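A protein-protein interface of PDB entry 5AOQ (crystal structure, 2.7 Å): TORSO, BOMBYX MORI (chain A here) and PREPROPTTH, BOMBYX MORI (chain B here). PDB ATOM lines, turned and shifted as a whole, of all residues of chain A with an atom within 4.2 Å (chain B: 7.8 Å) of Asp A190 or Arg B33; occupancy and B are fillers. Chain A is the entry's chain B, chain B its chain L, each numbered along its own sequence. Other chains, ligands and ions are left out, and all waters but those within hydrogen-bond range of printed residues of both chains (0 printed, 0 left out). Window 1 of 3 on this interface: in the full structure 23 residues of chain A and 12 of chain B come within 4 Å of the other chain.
The side-chain amino group of Lys A204 lies within salt-bridge range of the side-chain carboxylate of Glu B28 (2.9 Å).
OD2 of Asp A190 is in salt-bridge range of NH1 of Arg B33 (2.8 Å).
NH2 of Arg A73 lies within salt-bridge range of OE2 of Glu B28, 3.2 Å away.
Among the printed residues, pairs that only touch across the chains: His A227 with Ile B23 and Lys A229 with Arg B33.
Of the 9 printed residues of chain A, 5 touch a printed residue of chain B.
Hydrophobic or aromatic side chains of chain A within 4 Å of the printed part of chain B: His A227.
Printed residues of chain B that touch a printed residue of chain A: Ile B23, Glu B28 and Arg B33.
Among the printed residues, 5 pairs touch across the chains.
Asp A190 touches one residue of chain B.
Printed residues of chain B within 4 Å of Lys A204: Glu B28 (2.9 Å).
Printed residues of chain B within 4 Å of Lys A229: Arg B33 (3.95 Å).
Printed residues of chain A within 4 Å of Ile B23: His A227 (3.3 Å).
Asp B25 touches none of the printed residues of chain A.
Of the printed residues of chain A, Glu B28 touches Arg A73 and Lys A204.
Of chain A, only Asp A190 (2.8 Å) and Lys A229 (3.95 Å) come within 4 Å of Arg B33.
Ile B63 touches none of the printed residues of chain A.
The nearest residue of chain B that does not touch Asp A190 is Glu B28 (4.3 Å).
The nearest printed residue of chain A that does not touch Arg B33 is Arg A73 (4.7 Å).
The guanidinium group (NH2) of Arg A73 is in salt-bridge range of the side-chain carboxylate (OD1) of Asp A190 (2.7 Å).
The side-chain carboxylate of Asp B25 is in salt-bridge range of the guanidinium group of Arg B33.
The backbone NH (N) of Lys A229 sits at hydrogen-bond distance from the backbone carbonyl oxygen (O) of Asp A190, at 2.8 Å.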
ATOM      1  N   ARG A  73      -3.995 -10.051 -10.634  1.00  0.00           N
ATOM      2  CA  ARG A  73      -2.552  -9.832 -10.712  1.00  0.00           C
ATOM      3  C   ARG A  73      -2.081  -9.087  -9.476  1.00  0.00           C
ATOM      4  O   ARG A  73      -2.552  -7.987  -9.173  1.00  0.00           O
ATOM      5  CB  ARG A  73      -2.177  -9.065 -11.979  1.00  0.00           C
ATOM      6  CG  ARG A  73      -2.491  -9.828 -13.251  1.00  0.00           C
ATOM      7  CD  ARG A  73      -2.232  -8.995 -14.487  1.00  0.00           C
ATOM      8  NE  ARG A  73      -2.815  -9.616 -15.671  1.00  0.00           N
ATOM      9  CZ  ARG A  73      -2.773  -9.094 -16.891  1.00  0.00           C
ATOM     10  NH1 ARG A  73      -2.169  -7.934 -17.106  1.00  0.00           N
ATOM     11  NH2 ARG A  73      -3.337  -9.740 -17.900  1.00  0.00           N
ATOM     12  N   PHE A 189      -2.245  -4.101 -18.123  1.00  0.00           N
ATOM     13  CA  PHE A 189      -2.762  -4.069 -19.490  1.00  0.00           C
ATOM     14  C   PHE A 189      -2.398  -5.313 -20.291  1.00  0.00           C
ATOM     15  O   PHE A 189      -1.442  -6.017 -19.966  1.00  0.00           O
ATOM     16  CB  PHE A 189      -2.250  -2.830 -20.232  1.00  0.00           C
ATOM     17  CG  PHE A 189      -2.616  -1.531 -19.575  1.00  0.00           C
ATOM     18  CD1 PHE A 189      -3.913  -1.051 -19.634  1.00  0.00           C
ATOM     19  CD2 PHE A 189      -1.661  -0.784 -18.906  1.00  0.00           C
ATOM     20  CE1 PHE A 189      -4.252   0.146 -19.032  1.00  0.00           C
ATOM     21  CE2 PHE A 189      -1.994   0.413 -18.305  1.00  0.00           C
ATOM     22  CZ  PHE A 189      -3.290   0.880 -18.369  1.00  0.00           C
ATOM     23  N   ASP A 190      -3.180  -5.571 -21.336  1.00  0.00           N
ATOM     24  CA  ASP A 190      -2.881  -6.633 -22.293  1.00  0.00           C
ATOM     25  C   ASP A 190      -2.878  -6.056 -23.700  1.00  0.00           C
ATOM     26  O   ASP A 190      -3.883  -5.509 -24.152  1.00  0.00           O
ATOM     27  CB  ASP A 190      -3.901  -7.768 -22.188  1.00  0.00           C
ATOM     28  CG  ASP A 190      -3.753  -8.566 -20.911  1.00  0.00           C
ATOM     29  OD1 ASP A 190      -4.226  -8.096 -19.856  1.00  0.00           O
ATOM     30  OD2 ASP A 190      -3.159  -9.663 -20.961  1.00  0.00           O
ATOM     31  N   ILE A 191      -1.753  -6.195 -24.395  1.00  0.00           N
ATOM     32  CA  ILE A 191      -1.562  -5.546 -25.687  1.00  0.00           C
ATOM     33  C   ILE A 191      -1.374  -6.559 -26.806  1.00  0.00           C
ATOM     34  O   ILE A 191      -0.642  -7.540 -26.653  1.00  0.00           O
ATOM     35  CB  ILE A 191      -0.355  -4.585 -25.660  1.00  0.00           C
ATOM     36  CG1 ILE A 191      -0.555  -3.511 -24.589  1.00  0.00           C
ATOM     37  CG2 ILE A 191      -0.175  -3.902 -27.010  1.00  0.00           C
ATOM     38  CD1 ILE A 191      -0.088  -3.909 -23.205  1.00  0.00           C
ATOM     39  N   ALA A 203       1.590  -9.028 -25.779  1.00  0.00           N
ATOM     40  CA  ALA A 203       2.255  -8.911 -24.488  1.00  0.00           C
ATOM     41  C   ALA A 203       1.274  -8.585 -23.369  1.00  0.00           C
ATOM     42  O   ALA A 203       0.140  -8.161 -23.611  1.00  0.00           O
ATOM     43  CB  ALA A 203       3.344  -7.853 -24.552  1.00  0.00           C
ATOM     44  N   LYS A 204       1.742  -8.779 -22.140  1.00  0.00           N
ATOM     45  CA  LYS A 204       0.962  -8.525 -20.937  1.00  0.00           C
ATOM     46  C   LYS A 204       1.753  -7.604 -20.017  1.00  0.00           C
ATOM     47  O   LYS A 204       2.787  -7.999 -19.476  1.00  0.00           O
ATOM     48  CB  LYS A 204       0.633  -9.839 -20.226  1.00  0.00           C
ATOM     49  CG  LYS A 204      -0.250  -9.693 -18.997  1.00  0.00           C
ATOM     50  CD  LYS A 204      -0.384 -11.016 -18.249  1.00  0.00           C
ATOM     51  CE  LYS A 204      -1.080 -12.077 -19.088  1.00  0.00           C
ATOM     52  NZ  LYS A 204      -1.316 -13.327 -18.319  1.00  0.00           N
ATOM     53  N   HIS A 227      -4.386  -3.390 -30.511  1.00  0.00           N
ATOM     54  CA  HIS A 227      -5.441  -3.400 -29.507  1.00  0.00           C
ATOM     55  C   HIS A 227      -4.855  -3.357 -28.104  1.00  0.00           C
ATOM     56  O   HIS A 227      -3.958  -4.143 -27.769  1.00  0.00           O
ATOM     57  CB  HIS A 227      -6.321  -4.637 -29.669  1.00  0.00           C
ATOM     58  CG  HIS A 227      -6.733  -4.898 -31.082  1.00  0.00           C
ATOM     59  ND1 HIS A 227      -7.802  -4.262 -31.677  1.00  0.00           N
ATOM     60  CD2 HIS A 227      -6.211  -5.716 -32.024  1.00  0.00           C
ATOM     61  CE1 HIS A 227      -7.925  -4.686 -32.923  1.00  0.00           C
ATOM     62  NE2 HIS A 227      -6.972  -5.569 -33.159  1.00  0.00           N
ATOM     63  N   VAL A 228      -5.370  -2.434 -27.297  1.00  0.00           N
ATOM     64  CA  VAL A 228      -4.958  -2.291 -25.906  1.00  0.00           C
ATOM     65  C   VAL A 228      -6.125  -2.586 -24.969  1.00  0.00           C
ATOM     66  O   VAL A 228      -7.091  -1.823 -24.894  1.00  0.00           O
ATOM     67  CB  VAL A 228      -4.413  -0.877 -25.620  1.00  0.00           C
ATOM     68  CG1 VAL A 228      -4.037  -0.726 -24.148  1.00  0.00           C
ATOM     69  CG2 VAL A 228      -3.210  -0.590 -26.502  1.00  0.00           C
ATOM     70  N   LYS A 229      -6.023  -3.711 -24.269  1.00  0.00           N
ATOM     71  CA  LYS A 229      -7.012  -4.120 -23.281  1.00  0.00           C
ATOM     72  C   LYS A 229      -6.598  -3.629 -21.901  1.00  0.00           C
ATOM     73  O   LYS A 229      -5.493  -3.921 -21.435  1.00  0.00           O
ATOM     74  CB  LYS A 229      -7.166  -5.644 -23.277  1.00  0.00           C
ATOM     75  CG  LYS A 229      -8.122  -6.192 -22.223  1.00  0.00           C
ATOM     76  CD  LYS A 229      -9.562  -5.815 -22.523  1.00  0.00           C
ATOM     77  CE  LYS A 229     -10.504  -6.313 -21.439  1.00  0.00           C
ATOM     78  NZ  LYS A 229     -11.933  -6.092 -21.798  1.00  0.00           N
ATOM     79  N   ILE B  23      -7.714  -8.996 -35.151  1.00  0.00           N
ATOM     80  CA  ILE B  23      -7.361  -9.776 -33.966  1.00  0.00           C
ATOM     81  C   ILE B  23      -8.581 -10.341 -33.242  1.00  0.00           C
ATOM     82  O   ILE B  23      -9.588  -9.655 -33.058  1.00  0.00           O
ATOM     83  CB  ILE B  23      -6.545  -8.930 -32.965  1.00  0.00           C
ATOM     84  CG1 ILE B  23      -5.267  -8.403 -33.624  1.00  0.00           C
ATOM     85  CG2 ILE B  23      -6.200  -9.741 -31.715  1.00  0.00           C
ATOM     86  CD1 ILE B  23      -4.321  -9.486 -34.110  1.00  0.00           C
ATOM     87  N   GLU B  24      -8.467 -11.605 -32.839  1.00  0.00           N
ATOM     88  CA  GLU B  24      -9.483 -12.278 -32.035  1.00  0.00           C
ATOM     89  C   GLU B  24      -8.972 -12.492 -30.614  1.00  0.00           C
ATOM     90  O   GLU B  24      -7.974 -13.179 -30.412  1.00  0.00           O
ATOM     91  CB  GLU B  24      -9.858 -13.619 -32.666  1.00  0.00           C
ATOM     92  CG  GLU B  24     -10.976 -13.537 -33.690  1.00  0.00           C
ATOM     93  CD  GLU B  24     -12.338 -13.326 -33.055  1.00  0.00           C
ATOM     94  OE1 GLU B  24     -12.414 -13.222 -31.813  1.00  0.00           O
ATOM     95  OE2 GLU B  24     -13.337 -13.266 -33.802  1.00  0.00           O
ATOM     96  N   ASP B  25      -9.675 -11.930 -29.634  1.00  0.00           N
ATOM     97  CA  ASP B  25      -9.217 -11.952 -28.245  1.00  0.00           C
ATOM     98  C   ASP B  25      -9.391 -13.329 -27.604  1.00  0.00           C
ATOM     99  O   ASP B  25      -8.465 -13.850 -26.982  1.00  0.00           O
ATOM    100  CB  ASP B  25      -9.967 -10.895 -27.427  1.00  0.00           C
ATOM    101  CG  ASP B  25      -9.306 -10.608 -26.091  1.00  0.00           C
ATOM    102  OD1 ASP B  25      -9.070 -11.559 -25.317  1.00  0.00           O
ATOM    103  OD2 ASP B  25      -9.019  -9.425 -25.816  1.00  0.00           O
ATOM    104  N   LEU B  26     -10.583 -13.902 -27.742  1.00  0.00           N
ATOM    105  CA  LEU B  26     -10.893 -15.226 -27.195  1.00  0.00           C
ATOM    106  C   LEU B  26     -10.706 -15.324 -25.677  1.00  0.00           C
ATOM    107  O   LEU B  26     -10.675 -16.424 -25.121  1.00  0.00           O
ATOM    108  CB  LEU B  26     -10.031 -16.291 -27.883  1.00  0.00           C
ATOM    109  CG  LEU B  26     -10.270 -16.477 -29.382  1.00  0.00           C
ATOM    110  CD1 LEU B  26      -9.240 -17.434 -29.948  1.00  0.00           C
ATOM    111  CD2 LEU B  26     -11.677 -16.982 -29.660  1.00  0.00           C
ATOM    112  N   GLY B  27     -10.589 -14.182 -25.008  1.00  0.00           N
ATOM    113  CA  GLY B  27     -10.418 -14.154 -23.565  1.00  0.00           C
ATOM    114  C   GLY B  27      -9.065 -14.668 -23.107  1.00  0.00           C
ATOM    115  O   GLY B  27      -8.355 -15.339 -23.855  1.00  0.00           O
ATOM    116  N   GLU B  28      -8.715 -14.363 -21.860  1.00  0.00           N
ATOM    117  CA  GLU B  28      -7.418 -14.745 -21.309  1.00  0.00           C
ATOM    118  C   GLU B  28      -7.353 -16.223 -20.929  1.00  0.00           C
ATOM    119  O   GLU B  28      -6.271 -16.762 -20.698  1.00  0.00           O
ATOM    120  CB  GLU B  28      -7.099 -13.884 -20.083  1.00  0.00           C
ATOM    121  CG  GLU B  28      -5.654 -13.975 -19.619  1.00  0.00           C
ATOM    122  CD  GLU B  28      -5.331 -12.987 -18.517  1.00  0.00           C
ATOM    123  OE1 GLU B  28      -6.275 -12.407 -17.939  1.00  0.00           O
ATOM    124  OE2 GLU B  28      -4.132 -12.786 -18.233  1.00  0.00           O
ATOM    125  N   ASN B  29      -8.506 -16.882 -20.877  1.00  0.00           N
ATOM    126  CA  ASN B  29      -8.555 -18.293 -20.514  1.00  0.00           C
ATOM    127  C   ASN B  29      -7.938 -19.190 -21.583  1.00  0.00           C
ATOM    128  O   ASN B  29      -7.574 -20.334 -21.307  1.00  0.00           O
ATOM    129  CB  ASN B  29     -10.000 -18.719 -20.250  1.00  0.00           C
ATOM    130  CG  ASN B  29     -10.546 -18.159 -18.950  1.00  0.00           C
ATOM    131  OD1 ASN B  29      -9.904 -17.335 -18.297  1.00  0.00           O
ATOM    132  ND2 ASN B  29     -11.737 -18.604 -18.567  1.00  0.00           N
ATOM    133  N   SER B  30      -7.821 -18.666 -22.798  1.00  0.00           N
ATOM    134  CA  SER B  30      -7.220 -19.411 -23.899  1.00  0.00           C
ATOM    135  C   SER B  30      -5.705 -19.238 -23.905  1.00  0.00           C
ATOM    136  O   SER B  30      -5.204 -18.129 -23.708  1.00  0.00           O
ATOM    137  CB  SER B  30      -7.806 -18.950 -25.235  1.00  0.00           C
ATOM    138  OG  SER B  30      -9.209 -19.142 -25.269  1.00  0.00           O
ATOM    139  N   VAL B  31      -4.976 -20.329 -24.125  1.00  0.00           N
ATOM    140  CA  VAL B  31      -3.520 -20.258 -24.196  1.00  0.00           C
ATOM    141  C   VAL B  31      -3.114 -19.437 -25.417  1.00  0.00           C
ATOM    142  O   VAL B  31      -2.358 -18.474 -25.288  1.00  0.00           O
ATOM    143  CB  VAL B  31      -2.870 -21.663 -24.236  1.00  0.00           C
ATOM    144  CG1 VAL B  31      -1.391 -21.572 -24.609  1.00  0.00           C
ATOM    145  CG2 VAL B  31      -3.039 -22.359 -22.899  1.00  0.00           C
ATOM    146  N   PRO B  32      -3.614 -19.809 -26.609  1.00  0.00           N
ATOM    147  CA  PRO B  32      -3.466 -18.867 -27.720  1.00  0.00           C
ATOM    148  C   PRO B  32      -4.561 -17.816 -27.645  1.00  0.00           C
ATOM    149  O   PRO B  32      -5.634 -17.993 -28.223  1.00  0.00           O
ATOM    150  CB  PRO B  32      -3.620 -19.756 -28.953  1.00  0.00           C
ATOM    151  CG  PRO B  32      -4.547 -20.831 -28.503  1.00  0.00           C
ATOM    152  CD  PRO B  32      -4.223 -21.079 -27.049  1.00  0.00           C
ATOM    153  N   ARG B  33      -4.293 -16.735 -26.923  1.00  0.00           N
ATOM    154  CA  ARG B  33      -5.300 -15.712 -26.702  1.00  0.00           C
ATOM    155  C   ARG B  33      -5.613 -14.976 -27.996  1.00  0.00           C
ATOM    156  O   ARG B  33      -6.660 -15.194 -28.606  1.00  0.00           O
ATOM    157  CB  ARG B  33      -4.839 -14.728 -25.626  1.00  0.00           C
ATOM    158  CG  ARG B  33      -5.858 -13.650 -25.315  1.00  0.00           C
ATOM    159  CD  ARG B  33      -5.436 -12.798 -24.137  1.00  0.00           C
ATOM    160  NE  ARG B  33      -6.417 -11.759 -23.846  1.00  0.00           N
ATOM    161  CZ  ARG B  33      -6.369 -10.955 -22.789  1.00  0.00           C
ATOM    162  NH1 ARG B  33      -5.384 -11.071 -21.907  1.00  0.00           N
ATOM    163  NH2 ARG B  33      -7.308 -10.038 -22.610  1.00  0.00           N
ATOM    164  N   PHE B  34      -4.695 -14.116 -28.418  1.00  0.00           N
ATOM    165  CA  PHE B  34      -4.905 -13.307 -29.610  1.00  0.00           C
ATOM    166  C   PHE B  34      -4.684 -14.117 -30.885  1.00  0.00           C
ATOM    167  O   PHE B  34      -3.599 -14.657 -31.108  1.00  0.00           O
ATOM    168  CB  PHE B  34      -3.990 -12.087 -29.578  1.00  0.00           C
ATOM    169  CG  PHE B  34      -4.157 -11.250 -28.344  1.00  0.00           C
ATOM    170  CD1 PHE B  34      -5.197 -10.341 -28.246  1.00  0.00           C
ATOM    171  CD2 PHE B  34      -3.277 -11.374 -27.282  1.00  0.00           C
ATOM    172  CE1 PHE B  34      -5.357  -9.569 -27.110  1.00  0.00           C
ATOM    173  CE2 PHE B  34      -3.431 -10.604 -26.146  1.00  0.00           C
ATOM    174  CZ  PHE B  34      -4.472  -9.701 -26.059  1.00  0.00           C
ATOM    175  N   ILE B  35      -5.723 -14.186 -31.717  1.00  0.00           N
ATOM    176  CA  ILE B  35      -5.673 -14.919 -32.985  1.00  0.00           C
ATOM    177  C   ILE B  35      -5.716 -13.979 -34.187  1.00  0.00           C
ATOM    178  O   ILE B  35      -6.453 -12.993 -34.195  1.00  0.00           O
ATOM    179  CB  ILE B  35      -6.838 -15.938 -33.080  1.00  0.00           C
ATOM    180  CG1 ILE B  35      -6.408 -17.305 -32.546  1.00  0.00           C
ATOM    181  CG2 ILE B  35      -7.326 -16.109 -34.522  1.00  0.00           C
ATOM    182  CD1 ILE B  35      -5.745 -17.273 -31.182  1.00  0.00           C
ATOM    183  N   GLU B  36      -4.915 -14.305 -35.199  1.00  0.00           N
ATOM    184  CA  GLU B  36      -4.848 -13.524 -36.430  1.00  0.00           C
ATOM    185  C   GLU B  36      -5.938 -13.951 -37.408  1.00  0.00           C
ATOM    186  O   GLU B  36      -6.022 -15.122 -37.783  1.00  0.00           O
ATOM    187  CB  GLU B  36      -3.468 -13.679 -37.080  1.00  0.00           C
ATOM    188  CG  GLU B  36      -3.286 -12.904 -38.375  1.00  0.00           C
ATOM    189  CD  GLU B  36      -1.888 -13.056 -38.951  1.00  0.00           C
ATOM    190  OE1 GLU B  36      -0.986 -13.512 -38.218  1.00  0.00           O
ATOM    191  OE2 GLU B  36      -1.695 -12.727 -40.140  1.00  0.00           O
ATOM    192  N   ILE B  63      -7.746 -24.146 -30.251  1.00  0.00           N
ATOM    193  CA  ILE B  63      -7.455 -23.283 -29.110  1.00  0.00           C
ATOM    194  C   ILE B  63      -7.595 -24.071 -27.820  1.00  0.00           C
ATOM    195  O   ILE B  63      -8.454 -24.947 -27.701  1.00  0.00           O
ATOM    196  CB  ILE B  63      -8.385 -22.046 -29.069  1.00  0.00           C
ATOM    197  CG1 ILE B  63      -8.001 -21.061 -30.170  1.00  0.00           C
ATOM    198  CG2 ILE B  63      -8.309 -21.333 -27.721  1.00  0.00           C
ATOM    199  CD1 ILE B  63      -8.805 -21.221 -31.416  1.00  0.00           C
ATOM    200  N   LEU B  64      -6.737 -23.743 -26.861  1.00  0.00           N
ATOM    201  CA  LEU B  64      -6.710 -24.418 -25.575  1.00  0.00           C
ATOM    202  C   LEU B  64      -7.303 -23.539 -24.475  1.00  0.00           C
ATOM    203  O   LEU B  64      -6.610 -22.702 -23.897  1.00  0.00           O
ATOM    204  CB  LEU B  64      -5.273 -24.821 -25.235  1.00  0.00           C
ATOM    205  CG  LEU B  64      -5.070 -25.994 -24.275  1.00  0.00           C
ATOM    206  CD1 LEU B  64      -5.691 -27.276 -24.817  1.00  0.00           C
ATOM    207  CD2 LEU B  64      -3.587 -26.191 -24.020  1.00  0.00           C
ATOM    208  N   HIS B  90     -11.683 -23.988 -33.924  1.00  0.00           N
ATOM    209  CA  HIS B  90     -12.050 -22.603 -34.177  1.00  0.00           C
ATOM    210  C   HIS B  90     -11.805 -22.230 -35.638  1.00  0.00           C
ATOM    211  O   HIS B  90     -10.670 -21.954 -36.026  1.00  0.00           O
ATOM    212  CB  HIS B  90     -11.262 -21.685 -33.246  1.00  0.00           C
ATOM    213  CG  HIS B  90     -11.811 -20.296 -33.149  1.00  0.00           C
ATOM    214  ND1 HIS B  90     -11.115 -19.187 -33.579  1.00  0.00           N
ATOM    215  CD2 HIS B  90     -12.985 -19.835 -32.656  1.00  0.00           C
ATOM    216  CE1 HIS B  90     -11.840 -18.103 -33.361  1.00  0.00           C
ATOM    217  NE2 HIS B  90     -12.979 -18.470 -32.802  1.00  0.00           N
